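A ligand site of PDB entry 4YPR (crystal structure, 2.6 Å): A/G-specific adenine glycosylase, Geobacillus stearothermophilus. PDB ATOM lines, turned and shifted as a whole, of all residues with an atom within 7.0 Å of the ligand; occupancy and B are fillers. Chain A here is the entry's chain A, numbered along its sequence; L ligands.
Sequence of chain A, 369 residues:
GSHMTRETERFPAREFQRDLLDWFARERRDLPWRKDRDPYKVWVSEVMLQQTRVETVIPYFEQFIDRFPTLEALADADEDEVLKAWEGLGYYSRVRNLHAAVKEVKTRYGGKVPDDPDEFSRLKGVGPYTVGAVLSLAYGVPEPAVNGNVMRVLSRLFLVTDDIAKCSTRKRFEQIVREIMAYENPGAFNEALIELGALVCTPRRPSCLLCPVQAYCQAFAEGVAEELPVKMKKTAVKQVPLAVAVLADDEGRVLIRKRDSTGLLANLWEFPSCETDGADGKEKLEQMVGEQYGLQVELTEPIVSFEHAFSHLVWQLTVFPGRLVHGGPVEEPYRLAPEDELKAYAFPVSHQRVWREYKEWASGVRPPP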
ATOM      1  N   ARG A 152     -14.327  10.167 -18.555  1.00  0.00           N
ATOM      2  CA  ARG A 152     -15.761  10.317 -18.669  1.00  0.00           C
ATOM      3  C   ARG A 152     -16.369  10.419 -17.269  1.00  0.00           C
ATOM      4  O   ARG A 152     -17.101  11.381 -16.966  1.00  0.00           O
ATOM      5  CB  ARG A 152     -16.376   9.145 -19.436  1.00  0.00           C
ATOM      6  CG  ARG A 152     -17.871   9.317 -19.660  1.00  0.00           C
ATOM      7  CD  ARG A 152     -18.394   8.470 -20.792  1.00  0.00           C
ATOM      8  NE  ARG A 152     -18.236   7.060 -20.503  1.00  0.00           N
ATOM      9  CZ  ARG A 152     -17.315   6.290 -21.051  1.00  0.00           C
ATOM     10  NH1 ARG A 152     -16.486   6.773 -21.954  1.00  0.00           N
ATOM     11  NH2 ARG A 152     -17.251   5.021 -20.715  1.00  0.00           N
ATOM     12  N   VAL A 153     -16.044   9.437 -16.428  1.00  0.00           N
ATOM     13  CA  VAL A 153     -16.495   9.367 -15.032  1.00  0.00           C
ATOM     14  C   VAL A 153     -16.100  10.641 -14.298  1.00  0.00           C
ATOM     15  O   VAL A 153     -16.951  11.325 -13.726  1.00  0.00           O
ATOM     16  CB  VAL A 153     -15.897   8.128 -14.283  1.00  0.00           C
ATOM     17  CG1 VAL A 153     -16.159   8.204 -12.793  1.00  0.00           C
ATOM     18  CG2 VAL A 153     -16.475   6.837 -14.831  1.00  0.00           C
ATOM     19  N   LEU A 154     -14.813  10.971 -14.333  1.00  0.00           N
ATOM     20  CA  LEU A 154     -14.344  12.128 -13.603  1.00  0.00           C
ATOM     21  C   LEU A 154     -14.938  13.424 -14.189  1.00  0.00           C
ATOM     22  O   LEU A 154     -15.285  14.335 -13.417  1.00  0.00           O
ATOM     23  CB  LEU A 154     -12.818  12.179 -13.592  1.00  0.00           C
ATOM     24  CG  LEU A 154     -12.160  11.032 -12.815  1.00  0.00           C
ATOM     25  CD1 LEU A 154     -10.651  11.160 -12.828  1.00  0.00           C
ATOM     26  CD2 LEU A 154     -12.671  11.012 -11.400  1.00  0.00           C
ATOM     27  N   ARG A 156     -17.768  13.716 -15.457  1.00  0.00           N
ATOM     28  CA  ARG A 156     -19.120  13.807 -14.928  1.00  0.00           C
ATOM     29  C   ARG A 156     -19.183  14.081 -13.433  1.00  0.00           C
ATOM     30  O   ARG A 156     -19.988  14.909 -13.002  1.00  0.00           O
ATOM     31  CB  ARG A 156     -19.887  12.554 -15.268  1.00  0.00           C
ATOM     32  CG  ARG A 156     -20.329  12.605 -16.710  1.00  0.00           C
ATOM     33  CD  ARG A 156     -20.445  11.230 -17.280  1.00  0.00           C
ATOM     34  NE  ARG A 156     -20.947  11.321 -18.647  1.00  0.00           N
ATOM     35  CZ  ARG A 156     -21.450  10.307 -19.321  1.00  0.00           C
ATOM     36  NH1 ARG A 156     -21.512   9.107 -18.764  1.00  0.00           N
ATOM     37  NH2 ARG A 156     -21.876  10.503 -20.567  1.00  0.00           N
ATOM     38  N   LEU A 157     -18.337  13.424 -12.633  1.00  0.00           N
ATOM     39  CA  LEU A 157     -18.416  13.584 -11.177  1.00  0.00           C
ATOM     40  C   LEU A 157     -18.129  15.037 -10.814  1.00  0.00           C
ATOM     41  O   LEU A 157     -18.833  15.637 -10.015  1.00  0.00           O
ATOM     42  CB  LEU A 157     -17.431  12.675 -10.455  1.00  0.00           C
ATOM     43  CG  LEU A 157     -17.812  11.190 -10.398  1.00  0.00           C
ATOM     44  CD1 LEU A 157     -16.689  10.320  -9.777  1.00  0.00           C
ATOM     45  CD2 LEU A 157     -19.159  10.971  -9.702  1.00  0.00           C
ATOM     46  N   LEU A 196     -16.101   1.115 -13.614  1.00  0.00           N
ATOM     47  CA  LEU A 196     -17.319   1.939 -13.541  1.00  0.00           C
ATOM     48  C   LEU A 196     -17.579   2.654 -14.885  1.00  0.00           C
ATOM     49  O   LEU A 196     -18.689   2.622 -15.409  1.00  0.00           O
ATOM     50  CB  LEU A 196     -17.230   2.964 -12.396  1.00  0.00           C
ATOM     51  CG  LEU A 196     -18.506   3.806 -12.239  1.00  0.00           C
ATOM     52  CD1 LEU A 196     -19.636   3.004 -11.603  1.00  0.00           C
ATOM     53  CD2 LEU A 196     -18.259   5.050 -11.451  1.00  0.00           C
ATOM     54  N   VAL A 200     -20.958   1.099 -16.325  1.00  0.00           N
ATOM     55  CA  VAL A 200     -22.045   1.876 -15.725  1.00  0.00           C
ATOM     56  C   VAL A 200     -22.089   3.300 -16.292  1.00  0.00           C
ATOM     57  O   VAL A 200     -23.096   3.704 -16.877  1.00  0.00           O
ATOM     58  CB  VAL A 200     -21.878   1.920 -14.176  1.00  0.00           C
ATOM     59  CG1 VAL A 200     -22.916   2.822 -13.525  1.00  0.00           C
ATOM     60  CG2 VAL A 200     -21.932   0.529 -13.597  1.00  0.00           C
ATOM     61  N   CYS A 201     -21.013   4.058 -16.128  1.00  0.00           N
ATOM     62  CA  CYS A 201     -20.992   5.441 -16.565  1.00  0.00           C
ATOM     63  C   CYS A 201     -20.653   5.520 -18.061  1.00  0.00           C
ATOM     64  O   CYS A 201     -19.583   5.977 -18.479  1.00  0.00           O
ATOM     65  CB  CYS A 201     -20.005   6.241 -15.709  1.00  0.00           C
ATOM     66  SG  CYS A 201     -20.019   8.022 -16.029  1.00  0.00           S
ATOM     67  N   THR A 202     -21.591   5.076 -18.875  1.00  0.00           N
ATOM     68  CA  THR A 202     -21.339   4.845 -20.299  1.00  0.00           C
ATOM     69  C   THR A 202     -21.604   6.112 -21.096  1.00  0.00           C
ATOM     70  O   THR A 202     -22.259   7.026 -20.586  1.00  0.00           O
ATOM     71  CB  THR A 202     -22.191   3.679 -20.781  1.00  0.00           C
ATOM     72  OG1 THR A 202     -23.562   3.942 -20.497  1.00  0.00           O
ATOM     73  CG2 THR A 202     -21.750   2.421 -20.043  1.00  0.00           C
ATOM     74  N   PRO A 206     -25.886   6.649 -19.439  1.00  0.00           N
ATOM     75  CA  PRO A 206     -25.273   5.953 -18.308  1.00  0.00           C
ATOM     76  C   PRO A 206     -26.332   5.444 -17.349  1.00  0.00           C
ATOM     77  O   PRO A 206     -27.466   5.934 -17.358  1.00  0.00           O
ATOM     78  CB  PRO A 206     -24.400   7.039 -17.654  1.00  0.00           C
ATOM     79  CG  PRO A 206     -24.991   8.319 -18.064  1.00  0.00           C
ATOM     80  CD  PRO A 206     -25.482   8.079 -19.474  1.00  0.00           C
ATOM     81  N   SER A 207     -25.974   4.459 -16.546  1.00  0.00           N
ATOM     82  CA  SER A 207     -26.919   3.788 -15.677  1.00  0.00           C
ATOM     83  C   SER A 207     -26.887   4.396 -14.274  1.00  0.00           C
ATOM     84  O   SER A 207     -26.701   3.681 -13.275  1.00  0.00           O
ATOM     85  CB  SER A 207     -26.605   2.302 -15.612  1.00  0.00           C
ATOM     86  OG  SER A 207     -26.475   1.773 -16.906  1.00  0.00           O
ATOM     87  N   CYS A 208     -27.059   5.713 -14.232  1.00  0.00           N
ATOM     88  CA  CYS A 208     -26.949   6.475 -12.988  1.00  0.00           C
ATOM     89  C   CYS A 208     -27.817   5.898 -11.864  1.00  0.00           C
ATOM     90  O   CYS A 208     -27.407   5.882 -10.696  1.00  0.00           O
ATOM     91  CB  CYS A 208     -27.345   7.924 -13.228  1.00  0.00           C
ATOM     92  SG  CYS A 208     -26.736   8.732 -14.740  1.00  0.00           S
ATOM     93  N   LEU A 209     -29.000   5.424 -12.223  1.00  0.00           N
ATOM     94  CA  LEU A 209     -29.918   4.807 -11.265  1.00  0.00           C
ATOM     95  C   LEU A 209     -29.249   3.690 -10.493  1.00  0.00           C
ATOM     96  O   LEU A 209     -29.617   3.408  -9.347  1.00  0.00           O
ATOM     97  CB  LEU A 209     -31.139   4.284 -11.991  1.00  0.00           C
ATOM     98  CG  LEU A 209     -32.210   3.405 -11.302  1.00  0.00           C
ATOM     99  CD1 LEU A 209     -31.892   1.912 -11.321  1.00  0.00           C
ATOM    100  CD2 LEU A 209     -32.537   3.868  -9.908  1.00  0.00           C
ATOM    101  N   LEU A 210     -28.261   3.059 -11.116  1.00  0.00           N
ATOM    102  CA  LEU A 210     -27.580   1.932 -10.498  1.00  0.00           C
ATOM    103  C   LEU A 210     -26.172   2.272 -10.134  1.00  0.00           C
ATOM    104  O   LEU A 210     -25.373   1.382  -9.838  1.00  0.00           O
ATOM    105  CB  LEU A 210     -27.560   0.744 -11.438  1.00  0.00           C
ATOM    106  CG  LEU A 210     -28.940   0.142 -11.543  1.00  0.00           C
ATOM    107  CD1 LEU A 210     -28.929  -1.023 -12.528  1.00  0.00           C
ATOM    108  CD2 LEU A 210     -29.358  -0.275 -10.142  1.00  0.00           C
ATOM    109  N   CYS A 211     -25.845   3.561 -10.160  1.00  0.00           N
ATOM    110  CA  CYS A 211     -24.436   3.912 -10.024  1.00  0.00           C
ATOM    111  C   CYS A 211     -24.046   4.011  -8.562  1.00  0.00           C
ATOM    112  O   CYS A 211     -24.645   4.745  -7.821  1.00  0.00           O
ATOM    113  CB  CYS A 211     -24.116   5.218 -10.726  1.00  0.00           C
ATOM    114  SG  CYS A 211     -22.445   5.687 -10.308  1.00  0.00           S
ATOM    115  N   PRO A 212     -23.001   3.277  -8.158  1.00  0.00           N
ATOM    116  CA  PRO A 212     -22.551   3.313  -6.764  1.00  0.00           C
ATOM    117  C   PRO A 212     -22.192   4.696  -6.269  1.00  0.00           C
ATOM    118  O   PRO A 212     -22.115   4.869  -5.063  1.00  0.00           O
ATOM    119  CB  PRO A 212     -21.307   2.425  -6.774  1.00  0.00           C
ATOM    120  CG  PRO A 212     -20.851   2.464  -8.198  1.00  0.00           C
ATOM    121  CD  PRO A 212     -22.113   2.466  -9.000  1.00  0.00           C
ATOM    122  N   VAL A 213     -21.929   5.656  -7.155  1.00  0.00           N
ATOM    123  CA  VAL A 213     -21.422   6.944  -6.652  1.00  0.00           C
ATOM    124  C   VAL A 213     -22.282   8.111  -7.073  1.00  0.00           C
ATOM    125  O   VAL A 213     -21.845   9.259  -7.027  1.00  0.00           O
ATOM    126  CB  VAL A 213     -19.968   7.200  -7.092  1.00  0.00           C
ATOM    127  CG1 VAL A 213     -19.021   6.206  -6.407  1.00  0.00           C
ATOM    128  CG2 VAL A 213     -19.838   7.142  -8.613  1.00  0.00           C
ATOM    129  N   GLN A 214     -23.515   7.792  -7.448  1.00  0.00           N
ATOM    130  CA  GLN A 214     -24.503   8.780  -7.797  1.00  0.00           C
ATOM    131  C   GLN A 214     -24.513   9.983  -6.864  1.00  0.00           C
ATOM    132  O   GLN A 214     -24.640  11.131  -7.311  1.00  0.00           O
ATOM    133  CB  GLN A 214     -25.900   8.142  -7.814  1.00  0.00           C
ATOM    134  CG  GLN A 214     -26.975   9.137  -8.185  1.00  0.00           C
ATOM    135  CD  GLN A 214     -28.357   8.578  -7.957  1.00  0.00           C
ATOM    136  OE1 GLN A 214     -29.108   9.070  -7.099  1.00  0.00           O
ATOM    137  NE2 GLN A 214     -28.715   7.537  -8.725  1.00  0.00           N
ATOM    138  N   ALA A 215     -24.353   9.733  -5.560  1.00  0.00           N
ATOM    139  CA  ALA A 215     -24.499  10.810  -4.565  1.00  0.00           C
ATOM    140  C   ALA A 215     -23.410  11.852  -4.670  1.00  0.00           C
ATOM    141  O   ALA A 215     -23.569  12.965  -4.171  1.00  0.00           O
ATOM    142  CB  ALA A 215     -24.532  10.243  -3.160  1.00  0.00           C
ATOM    143  N   TYR A 216     -22.326  11.506  -5.351  1.00  0.00           N
ATOM    144  CA  TYR A 216     -21.165  12.376  -5.440  1.00  0.00           C
ATOM    145  C   TYR A 216     -21.125  13.095  -6.771  1.00  0.00           C
ATOM    146  O   TYR A 216     -20.282  13.942  -7.009  1.00  0.00           O
ATOM    147  CB  TYR A 216     -19.895  11.556  -5.265  1.00  0.00           C
ATOM    148  CG  TYR A 216     -19.957  10.686  -4.051  1.00  0.00           C
ATOM    149  CD1 TYR A 216     -20.545   9.438  -4.102  1.00  0.00           C
ATOM    150  CD2 TYR A 216     -19.469  11.122  -2.821  1.00  0.00           C
ATOM    151  CE1 TYR A 216     -20.623   8.632  -2.962  1.00  0.00           C
ATOM    152  CE2 TYR A 216     -19.537  10.331  -1.689  1.00  0.00           C
ATOM    153  CZ  TYR A 216     -20.118   9.094  -1.761  1.00  0.00           C
ATOM    154  OH  TYR A 216     -20.190   8.284  -0.645  1.00  0.00           O
ATOM    155  N   CYS A 217     -22.052  12.756  -7.648  1.00  0.00           N
ATOM    156  CA  CYS A 217     -21.902  13.205  -9.029  1.00  0.00           C
ATOM    157  C   CYS A 217     -22.607  14.532  -9.345  1.00  0.00           C
ATOM    158  O   CYS A 217     -23.828  14.661  -9.200  1.00  0.00           O
ATOM    159  CB  CYS A 217     -22.394  12.113  -9.962  1.00  0.00           C
ATOM    160  SG  CYS A 217     -22.259  12.651 -11.642  1.00  0.00           S
ATOM    161  N   GLN A 218     -21.830  15.506  -9.800  1.00  0.00           N
ATOM    162  CA  GLN A 218     -22.394  16.802 -10.145  1.00  0.00           C
ATOM    163  C   GLN A 218     -23.174  16.756 -11.427  1.00  0.00           C
ATOM    164  O   GLN A 218     -24.263  17.313 -11.502  1.00  0.00           O
ATOM    165  CB  GLN A 218     -21.312  17.859 -10.254  1.00  0.00           C
ATOM    166  CG  GLN A 218     -20.883  18.439  -8.925  1.00  0.00           C
ATOM    167  CD  GLN A 218     -19.674  19.316  -9.067  1.00  0.00           C
ATOM    168  OE1 GLN A 218     -19.669  20.260  -9.863  1.00  0.00           O
ATOM    169  NE2 GLN A 218     -18.621  19.009  -8.312  1.00  0.00           N
ATOM    170  N   ALA A 219     -22.609  16.108 -12.447  1.00  0.00           N
ATOM    171  CA  ALA A 219     -23.312  15.949 -13.721  1.00  0.00           C
ATOM    172  C   ALA A 219     -24.710  15.429 -13.465  1.00  0.00           C
ATOM    173  O   ALA A 219     -25.681  15.925 -14.054  1.00  0.00           O
ATOM    174  CB  ALA A 219     -22.570  15.004 -14.657  1.00  0.00           C
ATOM    175  N   PHE A 220     -24.811  14.444 -12.570  1.00  0.00           N
ATOM    176  CA  PHE A 220     -26.084  13.791 -12.334  1.00  0.00           C
ATOM    177  C   PHE A 220     -27.055  14.769 -11.727  1.00  0.00           C
ATOM    178  O   PHE A 220     -28.219  14.848 -12.133  1.00  0.00           O
ATOM    179  CB  PHE A 220     -25.939  12.589 -11.416  1.00  0.00           C
ATOM    180  CG  PHE A 220     -27.276  11.997 -11.018  1.00  0.00           C
ATOM    181  CD1 PHE A 220     -27.936  11.115 -11.866  1.00  0.00           C
ATOM    182  CD2 PHE A 220     -27.871  12.333  -9.807  1.00  0.00           C
ATOM    183  CE1 PHE A 220     -29.157  10.582 -11.509  1.00  0.00           C
ATOM    184  CE2 PHE A 220     -29.108  11.815  -9.444  1.00  0.00           C
ATOM    185  CZ  PHE A 220     -29.754  10.927 -10.309  1.00  0.00           C
ATOM    186  N   ALA A 221     -26.567  15.496 -10.720  1.00  0.00           N
ATOM    187  CA  ALA A 221     -27.397  16.445  -9.989  1.00  0.00           C
ATOM    188  C   ALA A 221     -27.876  17.590 -10.892  1.00  0.00           C
ATOM    189  O   ALA A 221     -28.959  18.122 -10.704  1.00  0.00           O
ATOM    190  CB  ALA A 221     -26.627  16.972  -8.827  1.00  0.00           C
ATOM    191  N   ALA A 225     -25.017  14.787 -17.438  1.00  0.00           N
ATOM    192  CA  ALA A 225     -24.065  13.710 -17.680  1.00  0.00           C
ATOM    193  C   ALA A 225     -23.866  13.437 -19.177  1.00  0.00           C
ATOM    194  O   ALA A 225     -22.742  13.271 -19.663  1.00  0.00           O
ATOM    195  CB  ALA A 225     -24.518  12.422 -16.962  1.00  0.00           C
ATOM    196  N   GLU A 226     -24.955  13.420 -19.919  1.00  0.00           N
ATOM    197  CA  GLU A 226     -24.856  13.010 -21.303  1.00  0.00           C
ATOM    198  C   GLU A 226     -24.180  14.042 -22.226  1.00  0.00           C
ATOM    199  O   GLU A 226     -23.909  13.756 -23.380  1.00  0.00           O
ATOM    200  CB  GLU A 226     -26.250  12.637 -21.813  1.00  0.00           C
ATOM    201  CG  GLU A 226     -26.317  11.185 -22.165  1.00  0.00           C
ATOM    202  CD  GLU A 226     -27.712  10.639 -22.256  1.00  0.00           C
ATOM    203  OE1 GLU A 226     -27.865   9.503 -22.743  1.00  0.00           O
ATOM    204  OE2 GLU A 226     -28.648  11.358 -21.824  1.00  0.00           O
HETATM  205 FE1  LIG L   1     -22.682   7.471 -11.858  1.00  0.00          FE
HETATM  206 FE2  LIG L   1     -24.454   8.695 -13.831  1.00  0.00          FE
HETATM  207 FE3  LIG L   1     -21.662   8.449 -14.376  1.00  0.00          FE
HETATM  208 FE4  LIG L   1     -22.517  10.314 -12.380  1.00  0.00          FE
HETATM  209  S1  LIG L   1     -22.977  10.162 -14.507  1.00  0.00           S
HETATM  210  S2  LIG L   1     -21.032   8.740 -12.317  1.00  0.00           S
HETATM  211  S3  LIG L   1     -24.153   9.043 -11.708  1.00  0.00           S
HETATM  212  S4  LIG L   1     -23.175   6.963 -13.909  1.00  0.00           S
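The side-chain sulfur (SG) of Cys 201 binds an iron atom (FE3) of the ligand (2.4 Å).
An iron atom (FE1) of the ligand is bound by the side-chain sulfur (SG) of Cys 211, at 2.4 Å.
FE2 of the ligand is bound by SG of Cys 208 (2.5 Å).
SG of Cys 217 binds FE4 of the ligand, 2.5 Å away.
NH1 of Arg 156 sits close to SG of Cys 201 (3.3 Å).
The backbone NH of Cys 201 lies within hydrogen-bond range of the backbone carbonyl oxygen of Leu 196, 2.8 Å away.
The side-chain sulfur (SG) of Cys 211 sits close to the backbone NH (N) of Gln 214.
The backbone NH (N) of Val 213 lies close to the side-chain sulfur (SG) of Cys 211 (3.2 Å).
O of Arg 156 sits close to SG of Cys 217.
The side-chain sulfur of Cys 217 sits close to the backbone NH of Phe 220, 3.3 Å away.
The backbone carbonyl oxygen (O) of Thr 202 lies within hydrogen-bond range of the guanidinium group (NH1) of Arg 156 (2.9 Å).
O of Leu 157 lies within hydrogen-bond range of N of Gln 218 (3.0 Å).
Arg 156 touches the ligand.
Leu 157 touches the ligand (CD2 to S2, 3.9 Å).
CB of Pro 206 touches S4 of the ligand (3.9 Å).
Gln 214 touches the ligand (CA to S3, 3.9 Å).
CB of Phe 220 touches S3 of the ligand, at 3.98 Å.
Ala 225 touches the ligand.
Ten residues have an atom within 4 Å of the ligand: Arg 156, Leu 157, Cys 201, Pro 206, Cys 208, Cys 211, Gln 214, Cys 217, Phe 220 and Ala 225.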
